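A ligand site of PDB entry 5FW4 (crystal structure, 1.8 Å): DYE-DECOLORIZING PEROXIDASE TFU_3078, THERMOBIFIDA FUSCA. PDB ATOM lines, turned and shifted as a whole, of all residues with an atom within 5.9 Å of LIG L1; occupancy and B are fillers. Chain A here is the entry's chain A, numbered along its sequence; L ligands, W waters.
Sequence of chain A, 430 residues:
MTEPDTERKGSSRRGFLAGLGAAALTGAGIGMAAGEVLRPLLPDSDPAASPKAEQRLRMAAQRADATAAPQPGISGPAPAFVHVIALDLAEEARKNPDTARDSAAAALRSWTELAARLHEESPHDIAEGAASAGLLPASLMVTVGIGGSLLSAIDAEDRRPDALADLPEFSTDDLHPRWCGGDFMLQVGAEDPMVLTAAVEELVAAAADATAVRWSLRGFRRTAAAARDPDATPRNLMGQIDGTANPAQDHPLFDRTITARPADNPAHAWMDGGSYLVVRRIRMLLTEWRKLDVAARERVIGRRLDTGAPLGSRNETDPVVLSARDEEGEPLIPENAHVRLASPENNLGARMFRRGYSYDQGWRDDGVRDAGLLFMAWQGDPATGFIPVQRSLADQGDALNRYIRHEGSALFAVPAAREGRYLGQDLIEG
FE1 of LIG L1 is bound by NE2 of His 338 (2.2 Å).
An oxygen (O1) of LIG L1 is in hydrogen-bond range of the backbone NH of Thr 244, at 3.2 Å.
O1 of LIG L1 is in salt-bridge range of NH2 of Arg 354 (3.2 Å).
An oxygen (O1) of LIG L1 sits at hydrogen-bond distance from the backbone NH (N) of Gly 243 (2.8 Å).
The backbone NH (N) of Ala 245 lies within hydrogen-bond range of an oxygen (O2) of LIG L1 (2.9 Å).
O2 of LG2 L2 binds FE1 of LIG L1 (2.4 Å).
The backbone carbonyl oxygen of Arg 280 is in hydrogen-bond range of the backbone NH of Phe 375 (2.8 Å).
A ring nitrogen (NE2) of His 406 lies within hydrogen-bond range of the side-chain amide oxygen (OE1) of Gln 390 (3.3 Å).
ND1 of His 406 is in hydrogen-bond range of NE of Arg 280 (3.0 Å).
The backbone NH (N) of Ile 282 sits at hydrogen-bond distance from the backbone carbonyl oxygen (O) of Leu 373 (2.9 Å).
The backbone NH (N) of Val 339 lies within hydrogen-bond range of the backbone carbonyl oxygen (O) of Ile 301, 3.1 Å away.
The side-chain amide oxygen (OE1) of Gln 240 sits at hydrogen-bond distance from the side-chain amide nitrogen (ND2) of Asn 236 (2.8 Å).
The side-chain amide nitrogen of Gln 240 lies close to the side-chain sulfur of Met 238 (3.8 Å).
The guanidinium group (NH1) of Arg 354 lies within hydrogen-bond range of the backbone carbonyl oxygen (O) of Met 352.
Merely in contact with LIG L1: Phe 375 (3.3 Å), Ile 241 (3.4 Å), Pro 344 (3.4 Å), Ala 342 (3.4 Å), Ile 282 (3.5 Å), Gln 240 (3.5 Å), Gln 390 (3.5 Å), Phe 386 (3.5 Å), Ile 404 (3.6 Å), Asn 236 (3.6 Å), Leu 400 (3.6 Å), Leu 373 (3.6 Å), Val 389 (3.7 Å), His 406 (3.7 Å), Val 339 (3.7 Å), Arg 303 (3.8 Å), Asp 242 (3.8 Å), Ser 343 (3.9 Å), Met 284 (3.9 Å), Leu 393 (3.9 Å), Met 352 (3.9 Å) and Ile 301 (3.97 Å).
Hydrophobic or aromatic side chains within 4 Å of LIG L1: Ala 245, Ile 282, Met 284, Ile 301, His 338, Val 339, Ala 342, Pro 344, Met 352, Leu 373, Phe 375, Phe 386, Val 389, Leu 393, Leu 400, Ile 404 and His 406.
27 residues have an atom within 4 Å of LIG L1: Asn 236, Gln 240, Ile 241, Asp 242, Gly 243, Thr 244, Ala 245, Ile 282, Met 284, Ile 301, Arg 303, His 338, Val 339, Ala 342, Ser 343, Pro 344, Met 352, Arg 354, Leu 373, Phe 375, Phe 386, Val 389, Gln 390, Leu 393, Leu 400, Ile 404 and His 406.
The nearest printed residue that does not touch LIG L1 is Met 238 (4.1 Å).
Water W2 bridges an oxygen (O2) of LIG L1 (2.6 Å) and the guanidinium group of Arg 303 (2.8 Å).
Water W3 lies within hydrogen-bond range of O4 of LIG L1 and NH2 of Arg 303.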
ATOM      1  N   ASN A 236     -27.059  -1.937   7.915  1.00  0.00           N
ATOM      2  CA  ASN A 236     -28.379  -2.140   7.284  1.00  0.00           C
ATOM      3  C   ASN A 236     -29.088  -3.371   7.823  1.00  0.00           C
ATOM      4  O   ASN A 236     -28.584  -3.977   8.812  1.00  0.00           O
ATOM      5  CB  ASN A 236     -28.320  -2.068   5.787  1.00  0.00           C
ATOM      6  CG  ASN A 236     -27.465  -3.212   5.209  1.00  0.00           C
ATOM      7  OD1 ASN A 236     -27.390  -4.222   5.865  1.00  0.00           O
ATOM      8  ND2 ASN A 236     -26.944  -3.044   4.037  1.00  0.00           N
ATOM      9  N   MET A 238     -29.596  -6.071   6.480  1.00  0.00           N
ATOM     10  CA  MET A 238     -28.785  -7.320   6.132  1.00  0.00           C
ATOM     11  C   MET A 238     -27.550  -7.493   7.013  1.00  0.00           C
ATOM     12  O   MET A 238     -26.706  -8.401   6.756  1.00  0.00           O
ATOM     13  CB  MET A 238     -28.449  -7.182   4.667  1.00  0.00           C
ATOM     14  CG  MET A 238     -29.416  -7.857   3.730  1.00  0.00           C
ATOM     15  SD  MET A 238     -29.090  -7.506   2.024  1.00  0.00           S
ATOM     16  CE  MET A 238     -30.429  -8.314   1.244  1.00  0.00           C
ATOM     17  N   GLN A 240     -24.978  -5.465   7.279  1.00  0.00           N
ATOM     18  CA  GLN A 240     -23.763  -4.993   6.641  1.00  0.00           C
ATOM     19  C   GLN A 240     -23.438  -3.595   7.065  1.00  0.00           C
ATOM     20  O   GLN A 240     -24.366  -2.787   7.259  1.00  0.00           O
ATOM     21  CB  GLN A 240     -23.924  -5.002   5.091  1.00  0.00           C
ATOM     22  CG  GLN A 240     -24.291  -6.378   4.518  1.00  0.00           C
ATOM     23  CD  GLN A 240     -25.247  -6.365   3.336  1.00  0.00           C
ATOM     24  OE1 GLN A 240     -25.858  -5.340   2.981  1.00  0.00           O
ATOM     25  NE2 GLN A 240     -25.402  -7.533   2.733  1.00  0.00           N
ATOM     26  N   ILE A 241     -22.157  -3.298   7.165  1.00  0.00           N
ATOM     27  CA  ILE A 241     -21.703  -1.923   7.243  1.00  0.00           C
ATOM     28  C   ILE A 241     -21.993  -1.236   5.889  1.00  0.00           C
ATOM     29  O   ILE A 241     -21.685  -1.749   4.820  1.00  0.00           O
ATOM     30  CB  ILE A 241     -20.255  -1.804   7.692  1.00  0.00           C
ATOM     31  CG1 ILE A 241     -20.127  -2.136   9.180  1.00  0.00           C
ATOM     32  CG2 ILE A 241     -19.665  -0.442   7.410  1.00  0.00           C
ATOM     33  CD1 ILE A 241     -18.757  -2.670   9.520  1.00  0.00           C
ATOM     34  N   ASP A 242     -22.658  -0.084   5.983  1.00  0.00           N
ATOM     35  CA  ASP A 242     -23.161   0.636   4.832  1.00  0.00           C
ATOM     36  C   ASP A 242     -22.649   2.071   4.837  1.00  0.00           C
ATOM     37  O   ASP A 242     -23.104   2.907   5.648  1.00  0.00           O
ATOM     38  CB  ASP A 242     -24.712   0.635   4.824  1.00  0.00           C
ATOM     39  CG  ASP A 242     -25.291   1.527   3.730  1.00  0.00           C
ATOM     40  OD1 ASP A 242     -24.610   1.686   2.686  1.00  0.00           O
ATOM     41  OD2 ASP A 242     -26.413   2.093   3.936  1.00  0.00           O
ATOM     42  N   GLY A 243     -21.737   2.376   3.909  1.00  0.00           N
ATOM     43  CA  GLY A 243     -21.203   3.744   3.742  1.00  0.00           C
ATOM     44  C   GLY A 243     -19.707   3.858   3.541  1.00  0.00           C
ATOM     45  O   GLY A 243     -19.208   4.916   3.149  1.00  0.00           O
ATOM     46  N   THR A 244     -18.990   2.765   3.728  1.00  0.00           N
ATOM     47  CA  THR A 244     -17.553   2.804   3.745  1.00  0.00           C
ATOM     48  C   THR A 244     -16.934   3.541   2.521  1.00  0.00           C
ATOM     49  O   THR A 244     -16.060   4.421   2.687  1.00  0.00           O
ATOM     50  CB  THR A 244     -17.018   1.374   3.900  1.00  0.00           C
ATOM     51  OG1 THR A 244     -17.581   0.791   5.084  1.00  0.00           O
ATOM     52  CG2 THR A 244     -15.488   1.348   3.973  1.00  0.00           C
ATOM     53  N   ALA A 245     -17.385   3.220   1.326  1.00  0.00           N
ATOM     54  CA  ALA A 245     -16.727   3.777   0.132  1.00  0.00           C
ATOM     55  C   ALA A 245     -17.213   5.147  -0.303  1.00  0.00           C
ATOM     56  O   ALA A 245     -16.743   5.639  -1.333  1.00  0.00           O
ATOM     57  CB  ALA A 245     -16.839   2.825  -1.039  1.00  0.00           C
ATOM     58  N   ASN A 246     -18.128   5.772   0.462  1.00  0.00           N
ATOM     59  CA  ASN A 246     -18.507   7.152   0.170  1.00  0.00           C
ATOM     60  C   ASN A 246     -17.270   8.032   0.190  1.00  0.00           C
ATOM     61  O   ASN A 246     -16.347   7.789   0.972  1.00  0.00           O
ATOM     62  CB  ASN A 246     -19.498   7.723   1.203  1.00  0.00           C
ATOM     63  CG  ASN A 246     -20.928   7.375   0.872  1.00  0.00           C
ATOM     64  OD1 ASN A 246     -21.311   7.250  -0.304  1.00  0.00           O
ATOM     65  ND2 ASN A 246     -21.739   7.219   1.913  1.00  0.00           N
ATOM     66  N   ARG A 280     -34.559   5.112  -4.139  1.00  0.00           N
ATOM     67  CA  ARG A 280     -35.105   3.817  -4.491  1.00  0.00           C
ATOM     68  C   ARG A 280     -35.570   3.130  -3.207  1.00  0.00           C
ATOM     69  O   ARG A 280     -34.843   3.087  -2.199  1.00  0.00           O
ATOM     70  CB  ARG A 280     -34.021   2.967  -5.217  1.00  0.00           C
ATOM     71  CG  ARG A 280     -33.400   3.613  -6.444  1.00  0.00           C
ATOM     72  CD  ARG A 280     -34.313   3.571  -7.675  1.00  0.00           C
ATOM     73  NE  ARG A 280     -34.225   2.263  -8.339  1.00  0.00           N
ATOM     74  CZ  ARG A 280     -34.577   1.987  -9.582  1.00  0.00           C
ATOM     75  NH1 ARG A 280     -35.061   2.908 -10.395  1.00  0.00           N
ATOM     76  NH2 ARG A 280     -34.398   0.744 -10.039  1.00  0.00           N
ATOM     77  N   ILE A 282     -36.010  -0.226  -1.793  1.00  0.00           N
ATOM     78  CA  ILE A 282     -35.473  -1.587  -2.153  1.00  0.00           C
ATOM     79  C   ILE A 282     -35.824  -2.576  -1.071  1.00  0.00           C
ATOM     80  O   ILE A 282     -35.265  -2.534   0.025  1.00  0.00           O
ATOM     81  CB  ILE A 282     -33.982  -1.575  -2.271  1.00  0.00           C
ATOM     82  CG1 ILE A 282     -33.491  -0.390  -3.062  1.00  0.00           C
ATOM     83  CG2 ILE A 282     -33.493  -2.889  -2.906  1.00  0.00           C
ATOM     84  CD1 ILE A 282     -34.007  -0.383  -4.420  1.00  0.00           C
ATOM     85  N   ARG A 283     -36.739  -3.468  -1.371  1.00  0.00           N
ATOM     86  CA  ARG A 283     -37.168  -4.490  -0.449  1.00  0.00           C
ATOM     87  C   ARG A 283     -36.043  -5.537  -0.356  1.00  0.00           C
ATOM     88  O   ARG A 283     -35.452  -5.867  -1.363  1.00  0.00           O
ATOM     89  CB  ARG A 283     -38.437  -5.139  -0.953  1.00  0.00           C
ATOM     90  CG  ARG A 283     -39.015  -6.191   0.014  1.00  0.00           C
ATOM     91  CD  ARG A 283     -40.364  -6.770  -0.349  1.00  0.00           C
ATOM     92  NE  ARG A 283     -40.502  -7.332  -1.692  1.00  0.00           N
ATOM     93  CZ  ARG A 283     -40.276  -8.606  -2.032  1.00  0.00           C
ATOM     94  NH1 ARG A 283     -39.920  -9.502  -1.131  1.00  0.00           N
ATOM     95  NH2 ARG A 283     -40.482  -8.981  -3.302  1.00  0.00           N
ATOM     96  N   MET A 284     -35.763  -5.972   0.875  1.00  0.00           N
ATOM     97  CA  MET A 284     -34.775  -7.068   1.162  1.00  0.00           C
ATOM     98  C   MET A 284     -35.487  -8.385   1.382  1.00  0.00           C
ATOM     99  O   MET A 284     -36.444  -8.475   2.135  1.00  0.00           O
ATOM    100  CB  MET A 284     -33.956  -6.702   2.397  1.00  0.00           C
ATOM    101  CG  MET A 284     -33.014  -5.541   2.165  1.00  0.00           C
ATOM    102  SD  MET A 284     -32.232  -5.077   3.633  1.00  0.00           S
ATOM    103  CE  MET A 284     -30.962  -4.024   3.145  1.00  0.00           C
ATOM    104  N   ILE A 301     -21.443  -9.449  -1.176  1.00  0.00           N
ATOM    105  CA  ILE A 301     -21.045  -8.011  -1.177  1.00  0.00           C
ATOM    106  C   ILE A 301     -19.564  -7.815  -1.491  1.00  0.00           C
ATOM    107  O   ILE A 301     -19.208  -6.909  -2.223  1.00  0.00           O
ATOM    108  CB  ILE A 301     -21.245  -7.340   0.175  1.00  0.00           C
ATOM    109  CG1 ILE A 301     -22.743  -7.269   0.531  1.00  0.00           C
ATOM    110  CG2 ILE A 301     -20.533  -5.979   0.206  1.00  0.00           C
ATOM    111  CD1 ILE A 301     -23.591  -6.410  -0.376  1.00  0.00           C
ATOM    112  N   ARG A 303     -17.381  -7.723   1.189  1.00  0.00           N
ATOM    113  CA  ARG A 303     -16.832  -7.263   2.444  1.00  0.00           C
ATOM    114  C   ARG A 303     -17.373  -8.130   3.574  1.00  0.00           C
ATOM    115  O   ARG A 303     -18.402  -8.791   3.417  1.00  0.00           O
ATOM    116  CB  ARG A 303     -17.153  -5.790   2.652  1.00  0.00           C
ATOM    117  CG  ARG A 303     -16.432  -4.845   1.708  1.00  0.00           C
ATOM    118  CD  ARG A 303     -16.950  -3.433   1.935  1.00  0.00           C
ATOM    119  NE  ARG A 303     -16.211  -2.365   1.247  1.00  0.00           N
ATOM    120  CZ  ARG A 303     -15.120  -1.759   1.697  1.00  0.00           C
ATOM    121  NH1 ARG A 303     -14.528  -2.099   2.848  1.00  0.00           N
ATOM    122  NH2 ARG A 303     -14.603  -0.791   0.967  1.00  0.00           N
ATOM    123  N   HIS A 338     -21.070  -7.301  -5.240  1.00  0.00           N
ATOM    124  CA  HIS A 338     -21.668  -6.004  -5.314  1.00  0.00           C
ATOM    125  C   HIS A 338     -20.628  -4.880  -5.448  1.00  0.00           C
ATOM    126  O   HIS A 338     -20.664  -4.118  -6.403  1.00  0.00           O
ATOM    127  CB  HIS A 338     -22.494  -5.823  -4.055  1.00  0.00           C
ATOM    128  CG  HIS A 338     -23.198  -4.515  -3.996  1.00  0.00           C
ATOM    129  ND1 HIS A 338     -24.223  -4.172  -4.839  1.00  0.00           N
ATOM    130  CD2 HIS A 338     -23.041  -3.473  -3.154  1.00  0.00           C
ATOM    131  CE1 HIS A 338     -24.658  -2.958  -4.544  1.00  0.00           C
ATOM    132  NE2 HIS A 338     -23.943  -2.519  -3.524  1.00  0.00           N
ATOM    133  N   VAL A 339     -19.716  -4.792  -4.494  1.00  0.00           N
ATOM    134  CA  VAL A 339     -18.694  -3.742  -4.499  1.00  0.00           C
ATOM    135  C   VAL A 339     -17.758  -3.810  -5.713  1.00  0.00           C
ATOM    136  O   VAL A 339     -17.187  -2.796  -6.114  1.00  0.00           O
ATOM    137  CB  VAL A 339     -17.866  -3.694  -3.184  1.00  0.00           C
ATOM    138  CG1 VAL A 339     -18.777  -3.713  -1.970  1.00  0.00           C
ATOM    139  CG2 VAL A 339     -16.865  -4.824  -3.105  1.00  0.00           C
ATOM    140  N   ALA A 342     -20.160  -2.356  -8.565  1.00  0.00           N
ATOM    141  CA  ALA A 342     -20.581  -0.980  -8.239  1.00  0.00           C
ATOM    142  C   ALA A 342     -19.409   0.023  -8.225  1.00  0.00           C
ATOM    143  O   ALA A 342     -19.630   1.235  -8.178  1.00  0.00           O
ATOM    144  CB  ALA A 342     -21.311  -0.957  -6.884  1.00  0.00           C
ATOM    145  N   SER A 343     -18.174  -0.463  -8.282  1.00  0.00           N
ATOM    146  CA  SER A 343     -17.001   0.389  -8.108  1.00  0.00           C
ATOM    147  C   SER A 343     -16.877   1.373  -9.241  1.00  0.00           C
ATOM    148  O   SER A 343     -17.086   1.005 -10.392  1.00  0.00           O
ATOM    149  CB  SER A 343     -15.714  -0.467  -8.103  1.00  0.00           C
ATOM    150  OG  SER A 343     -15.646  -1.217  -9.312  1.00  0.00           O
ATOM    151  N   PRO A 344     -16.481   2.625  -8.956  1.00  0.00           N
ATOM    152  CA  PRO A 344     -16.220   3.590 -10.025  1.00  0.00           C
ATOM    153  C   PRO A 344     -15.340   2.996 -11.100  1.00  0.00           C
ATOM    154  O   PRO A 344     -15.547   3.257 -12.277  1.00  0.00           O
ATOM    155  CB  PRO A 344     -15.465   4.713  -9.323  1.00  0.00           C
ATOM    156  CG  PRO A 344     -15.944   4.645  -7.926  1.00  0.00           C
ATOM    157  CD  PRO A 344     -16.200   3.202  -7.631  1.00  0.00           C
ATOM    158  N   MET A 352     -21.030   8.283  -6.553  1.00  0.00           N
ATOM    159  CA  MET A 352     -22.198   8.888  -5.897  1.00  0.00           C
ATOM    160  C   MET A 352     -21.949   8.887  -4.418  1.00  0.00           C
ATOM    161  O   MET A 352     -21.036   8.224  -3.940  1.00  0.00           O
ATOM    162  CB  MET A 352     -23.477   8.125  -6.260  1.00  0.00           C
ATOM    163  CG  MET A 352     -23.643   6.774  -5.575  1.00  0.00           C
ATOM    164  SD  MET A 352     -24.709   5.655  -6.472  1.00  0.00           S
ATOM    165  CE  MET A 352     -23.562   5.095  -7.776  1.00  0.00           C
ATOM    166  N   ARG A 354     -23.936   7.966  -1.041  1.00  0.00           N
ATOM    167  CA  ARG A 354     -25.069   7.189  -0.599  1.00  0.00           C
ATOM    168  C   ARG A 354     -25.394   7.558   0.827  1.00  0.00           C
ATOM    169  O   ARG A 354     -24.521   7.523   1.697  1.00  0.00           O
ATOM    170  CB  ARG A 354     -24.745   5.694  -0.738  1.00  0.00           C
ATOM    171  CG  ARG A 354     -24.808   5.259  -2.188  1.00  0.00           C
ATOM    172  CD  ARG A 354     -23.879   4.077  -2.568  1.00  0.00           C
ATOM    173  NE  ARG A 354     -22.825   3.748  -1.624  1.00  0.00           N
ATOM    174  CZ  ARG A 354     -21.574   4.200  -1.612  1.00  0.00           C
ATOM    175  NH1 ARG A 354     -21.053   5.090  -2.520  1.00  0.00           N
ATOM    176  NH2 ARG A 354     -20.789   3.721  -0.638  1.00  0.00           N
ATOM    177  N   LEU A 373     -34.115  -1.260   2.377  1.00  0.00           N
ATOM    178  CA  LEU A 373     -33.244  -0.098   2.277  1.00  0.00           C
ATOM    179  C   LEU A 373     -33.957   0.990   1.486  1.00  0.00           C
ATOM    180  O   LEU A 373     -34.328   0.816   0.289  1.00  0.00           O
ATOM    181  CB  LEU A 373     -31.926  -0.442   1.571  1.00  0.00           C
ATOM    182  CG  LEU A 373     -30.874   0.666   1.402  1.00  0.00           C
ATOM    183  CD1 LEU A 373     -30.386   1.082   2.786  1.00  0.00           C
ATOM    184  CD2 LEU A 373     -29.691   0.223   0.519  1.00  0.00           C
ATOM    185  N   PHE A 375     -32.904   3.549  -0.197  1.00  0.00           N
ATOM    186  CA  PHE A 375     -31.625   3.923  -0.751  1.00  0.00           C
ATOM    187  C   PHE A 375     -31.679   5.332  -1.315  1.00  0.00           C
ATOM    188  O   PHE A 375     -32.608   5.674  -2.016  1.00  0.00           O
ATOM    189  CB  PHE A 375     -31.311   2.956  -1.884  1.00  0.00           C
ATOM    190  CG  PHE A 375     -30.147   3.359  -2.739  1.00  0.00           C
ATOM    191  CD1 PHE A 375     -30.301   4.260  -3.790  1.00  0.00           C
ATOM    192  CD2 PHE A 375     -28.909   2.712  -2.572  1.00  0.00           C
ATOM    193  CE1 PHE A 375     -29.216   4.583  -4.602  1.00  0.00           C
ATOM    194  CE2 PHE A 375     -27.829   3.063  -3.363  1.00  0.00           C
ATOM    195  CZ  PHE A 375     -27.973   3.975  -4.384  1.00  0.00           C
ATOM    196  N   PHE A 386     -25.544   7.332 -10.251  1.00  0.00           N
ATOM    197  CA  PHE A 386     -26.505   6.223 -10.131  1.00  0.00           C
ATOM    198  C   PHE A 386     -26.772   5.399 -11.413  1.00  0.00           C
ATOM    199  O   PHE A 386     -26.770   4.155 -11.342  1.00  0.00           O
ATOM    200  CB  PHE A 386     -27.851   6.738  -9.626  1.00  0.00           C
ATOM    201  CG  PHE A 386     -28.890   5.678  -9.524  1.00  0.00           C
ATOM    202  CD1 PHE A 386     -28.925   4.853  -8.405  1.00  0.00           C
ATOM    203  CD2 PHE A 386     -29.852   5.517 -10.497  1.00  0.00           C
ATOM    204  CE1 PHE A 386     -29.898   3.869  -8.286  1.00  0.00           C
ATOM    205  CE2 PHE A 386     -30.843   4.545 -10.380  1.00  0.00           C
ATOM    206  CZ  PHE A 386     -30.849   3.706  -9.270  1.00  0.00           C
ATOM    207  N   VAL A 389     -24.080   2.898 -12.874  1.00  0.00           N
ATOM    208  CA  VAL A 389     -23.792   1.923 -11.835  1.00  0.00           C
ATOM    209  C   VAL A 389     -24.930   0.929 -11.692  1.00  0.00           C
ATOM    210  O   VAL A 389     -24.697  -0.305 -11.650  1.00  0.00           O
ATOM    211  CB  VAL A 389     -23.466   2.589 -10.508  1.00  0.00           C
ATOM    212  CG1 VAL A 389     -23.333   1.595  -9.361  1.00  0.00           C
ATOM    213  CG2 VAL A 389     -22.219   3.429 -10.644  1.00  0.00           C
ATOM    214  N   GLN A 390     -26.155   1.425 -11.635  1.00  0.00           N
ATOM    215  CA  GLN A 390     -27.284   0.521 -11.498  1.00  0.00           C
ATOM    216  C   GLN A 390     -27.422  -0.368 -12.717  1.00  0.00           C
ATOM    217  O   GLN A 390     -27.828  -1.515 -12.574  1.00  0.00           O
ATOM    218  CB  GLN A 390     -28.599   1.254 -11.265  1.00  0.00           C
ATOM    219  CG  GLN A 390     -29.837   0.352 -11.304  1.00  0.00           C
ATOM    220  CD  GLN A 390     -29.927  -0.663 -10.191  1.00  0.00           C
ATOM    221  OE1 GLN A 390     -30.860  -1.464 -10.153  1.00  0.00           O
ATOM    222  NE2 GLN A 390     -28.978  -0.655  -9.268  1.00  0.00           N
ATOM    223  N   LEU A 393     -25.181  -3.187 -12.329  1.00  0.00           N
ATOM    224  CA  LEU A 393     -25.632  -4.124 -11.319  1.00  0.00           C
ATOM    225  C   LEU A 393     -26.761  -4.953 -11.866  1.00  0.00           C
ATOM    226  O   LEU A 393     -26.805  -6.146 -11.635  1.00  0.00           O
ATOM    227  CB  LEU A 393     -26.093  -3.439 -10.038  1.00  0.00           C
ATOM    228  CG  LEU A 393     -25.128  -2.600  -9.222  1.00  0.00           C
ATOM    229  CD1 LEU A 393     -25.806  -2.055  -7.970  1.00  0.00           C
ATOM    230  CD2 LEU A 393     -23.861  -3.373  -8.829  1.00  0.00           C
ATOM    231  N   LEU A 400     -26.090  -9.636  -5.355  1.00  0.00           N
ATOM    232  CA  LEU A 400     -27.121  -9.078  -4.485  1.00  0.00           C
ATOM    233  C   LEU A 400     -28.543  -9.057  -5.073  1.00  0.00           C
ATOM    234  O   LEU A 400     -29.534  -9.073  -4.306  1.00  0.00           O
ATOM    235  CB  LEU A 400     -26.695  -7.681  -4.089  1.00  0.00           C
ATOM    236  CG  LEU A 400     -27.586  -6.855  -3.127  1.00  0.00           C
ATOM    237  CD1 LEU A 400     -27.747  -7.554  -1.789  1.00  0.00           C
ATOM    238  CD2 LEU A 400     -26.879  -5.528  -2.940  1.00  0.00           C
ATOM    239  N   ILE A 404     -32.826  -8.741  -3.349  1.00  0.00           N
ATOM    240  CA  ILE A 404     -33.452  -7.406  -3.337  1.00  0.00           C
ATOM    241  C   ILE A 404     -34.438  -7.189  -4.479  1.00  0.00           C
ATOM    242  O   ILE A 404     -34.292  -7.783  -5.539  1.00  0.00           O
ATOM    243  CB  ILE A 404     -32.411  -6.248  -3.412  1.00  0.00           C
ATOM    244  CG1 ILE A 404     -31.777  -6.158  -4.813  1.00  0.00           C
ATOM    245  CG2 ILE A 404     -31.441  -6.334  -2.255  1.00  0.00           C
ATOM    246  CD1 ILE A 404     -30.643  -5.170  -4.949  1.00  0.00           C
ATOM    247  N   HIS A 406     -36.171  -3.768  -6.411  1.00  0.00           N
ATOM    248  CA  HIS A 406     -36.443  -2.345  -6.546  1.00  0.00           C
ATOM    249  C   HIS A 406     -37.947  -2.078  -6.744  1.00  0.00           C
ATOM    250  O   HIS A 406     -38.486  -2.299  -7.821  1.00  0.00           O
ATOM    251  CB  HIS A 406     -35.621  -1.785  -7.713  1.00  0.00           C
ATOM    252  CG  HIS A 406     -34.163  -1.651  -7.432  1.00  0.00           C
ATOM    253  ND1 HIS A 406     -33.565  -0.434  -7.187  1.00  0.00           N
ATOM    254  CD2 HIS A 406     -33.166  -2.577  -7.370  1.00  0.00           C
ATOM    255  CE1 HIS A 406     -32.280  -0.603  -6.977  1.00  0.00           C
ATOM    256  NE2 HIS A 406     -31.995  -1.896  -7.097  1.00  0.00           N
HETATM  257  C1  LIG L   1     -21.306  -0.395  -1.575  1.00  0.00           C
HETATM  258  C2  LIG L   1     -25.171  -2.679   0.238  1.00  0.00           C
HETATM  259  C3  LIG L   1     -27.788  -1.031  -3.480  1.00  0.00           C
HETATM  260  C4  LIG L   1     -23.991   1.474  -5.131  1.00  0.00           C
HETATM  261  C5  LIG L   1     -22.136  -1.149  -0.776  1.00  0.00           C
HETATM  262  C6  LIG L   1     -21.701  -1.842   0.372  1.00  0.00           C
HETATM  263  C7  LIG L   1     -22.773  -2.492   0.858  1.00  0.00           C
HETATM  264  C8  LIG L   1     -23.876  -2.210   0.046  1.00  0.00           C
HETATM  265  C9  LIG L   1     -22.836  -3.335   2.074  1.00  0.00           C
HETATM  266  C10 LIG L   1     -20.291  -1.895   0.911  1.00  0.00           C
HETATM  267  C11 LIG L   1     -19.996  -0.814   1.954  1.00  0.00           C
HETATM  268  C12 LIG L   1     -19.898   0.542   1.320  1.00  0.00           C
HETATM  269  O1  LIG L   1     -20.856   1.353   1.513  1.00  0.00           O
HETATM  270  O2  LIG L   1     -18.889   0.850   0.637  1.00  0.00           O
HETATM  271  C13 LIG L   1     -26.233  -2.416  -0.652  1.00  0.00           C
HETATM  272  C14 LIG L   1     -27.534  -2.923  -0.481  1.00  0.00           C
HETATM  273  C15 LIG L   1     -28.305  -2.462  -1.521  1.00  0.00           C
HETATM  274  C16 LIG L   1     -27.399  -1.646  -2.322  1.00  0.00           C
HETATM  275  C17 LIG L   1     -27.985  -3.788   0.661  1.00  0.00           C
HETATM  276  C18 LIG L   1     -29.735  -2.621  -1.820  1.00  0.00           C
HETATM  277  C19 LIG L   1     -30.617  -3.130  -0.961  1.00  0.00           C
HETATM  278  C20 LIG L   1     -27.006  -0.207  -4.248  1.00  0.00           C
HETATM  279  C21 LIG L   1     -27.435   0.457  -5.373  1.00  0.00           C
HETATM  280  C22 LIG L   1     -26.348   1.190  -5.837  1.00  0.00           C
HETATM  281  C23 LIG L   1     -25.251   0.939  -4.974  1.00  0.00           C
HETATM  282  C24 LIG L   1     -28.860   0.352  -5.883  1.00  0.00           C
HETATM  283  C25 LIG L   1     -26.146   2.034  -7.000  1.00  0.00           C
HETATM  284  C26 LIG L   1     -26.896   1.968  -8.055  1.00  0.00           C
HETATM  285  C27 LIG L   1     -22.961   1.117  -4.239  1.00  0.00           C
HETATM  286  C28 LIG L   1     -21.604   1.656  -4.408  1.00  0.00           C
HETATM  287  C29 LIG L   1     -20.858   1.124  -3.414  1.00  0.00           C
HETATM  288  C30 LIG L   1     -21.770   0.257  -2.673  1.00  0.00           C
HETATM  289  C31 LIG L   1     -21.117   2.637  -5.460  1.00  0.00           C
HETATM  290  C32 LIG L   1     -19.389   1.400  -3.165  1.00  0.00           C
HETATM  291  C33 LIG L   1     -18.557   0.514  -4.098  1.00  0.00           C
HETATM  292  C34 LIG L   1     -17.085   0.857  -3.990  1.00  0.00           C
HETATM  293  O3  LIG L   1     -16.595   1.842  -4.564  1.00  0.00           O
HETATM  294  O4  LIG L   1     -16.365   0.137  -3.272  1.00  0.00           O
HETATM  295  N1  LIG L   1     -23.481  -1.382  -0.975  1.00  0.00           N
HETATM  296  N2  LIG L   1     -26.192  -1.663  -1.742  1.00  0.00           N
HETATM  297  N3  LIG L   1     -25.675   0.055  -4.048  1.00  0.00           N
HETATM  298  N4  LIG L   1     -23.040   0.276  -3.174  1.00  0.00           N
HETATM  299 FE1  LIG L   1     -24.530  -0.706  -2.526  1.00  0.00          FE
HETATM  300  O1  LG2 L   2     -25.922   1.235  -0.114  1.00  0.00           O
HETATM  301  O2  LG2 L   2     -25.625   1.108  -1.308  1.00  0.00           O
HETATM  302  O   HOH W   1     -19.592   4.137  -8.002  1.00  0.00           O
HETATM  303  O   HOH W   2     -17.272  -0.723  -0.701  1.00  0.00           O
HETATM  304  O   HOH W   3     -14.101   0.719  -1.752  1.00  0.00           O
HETATM  305  O   HOH W   4     -19.578   5.718  -5.685  1.00  0.00           O
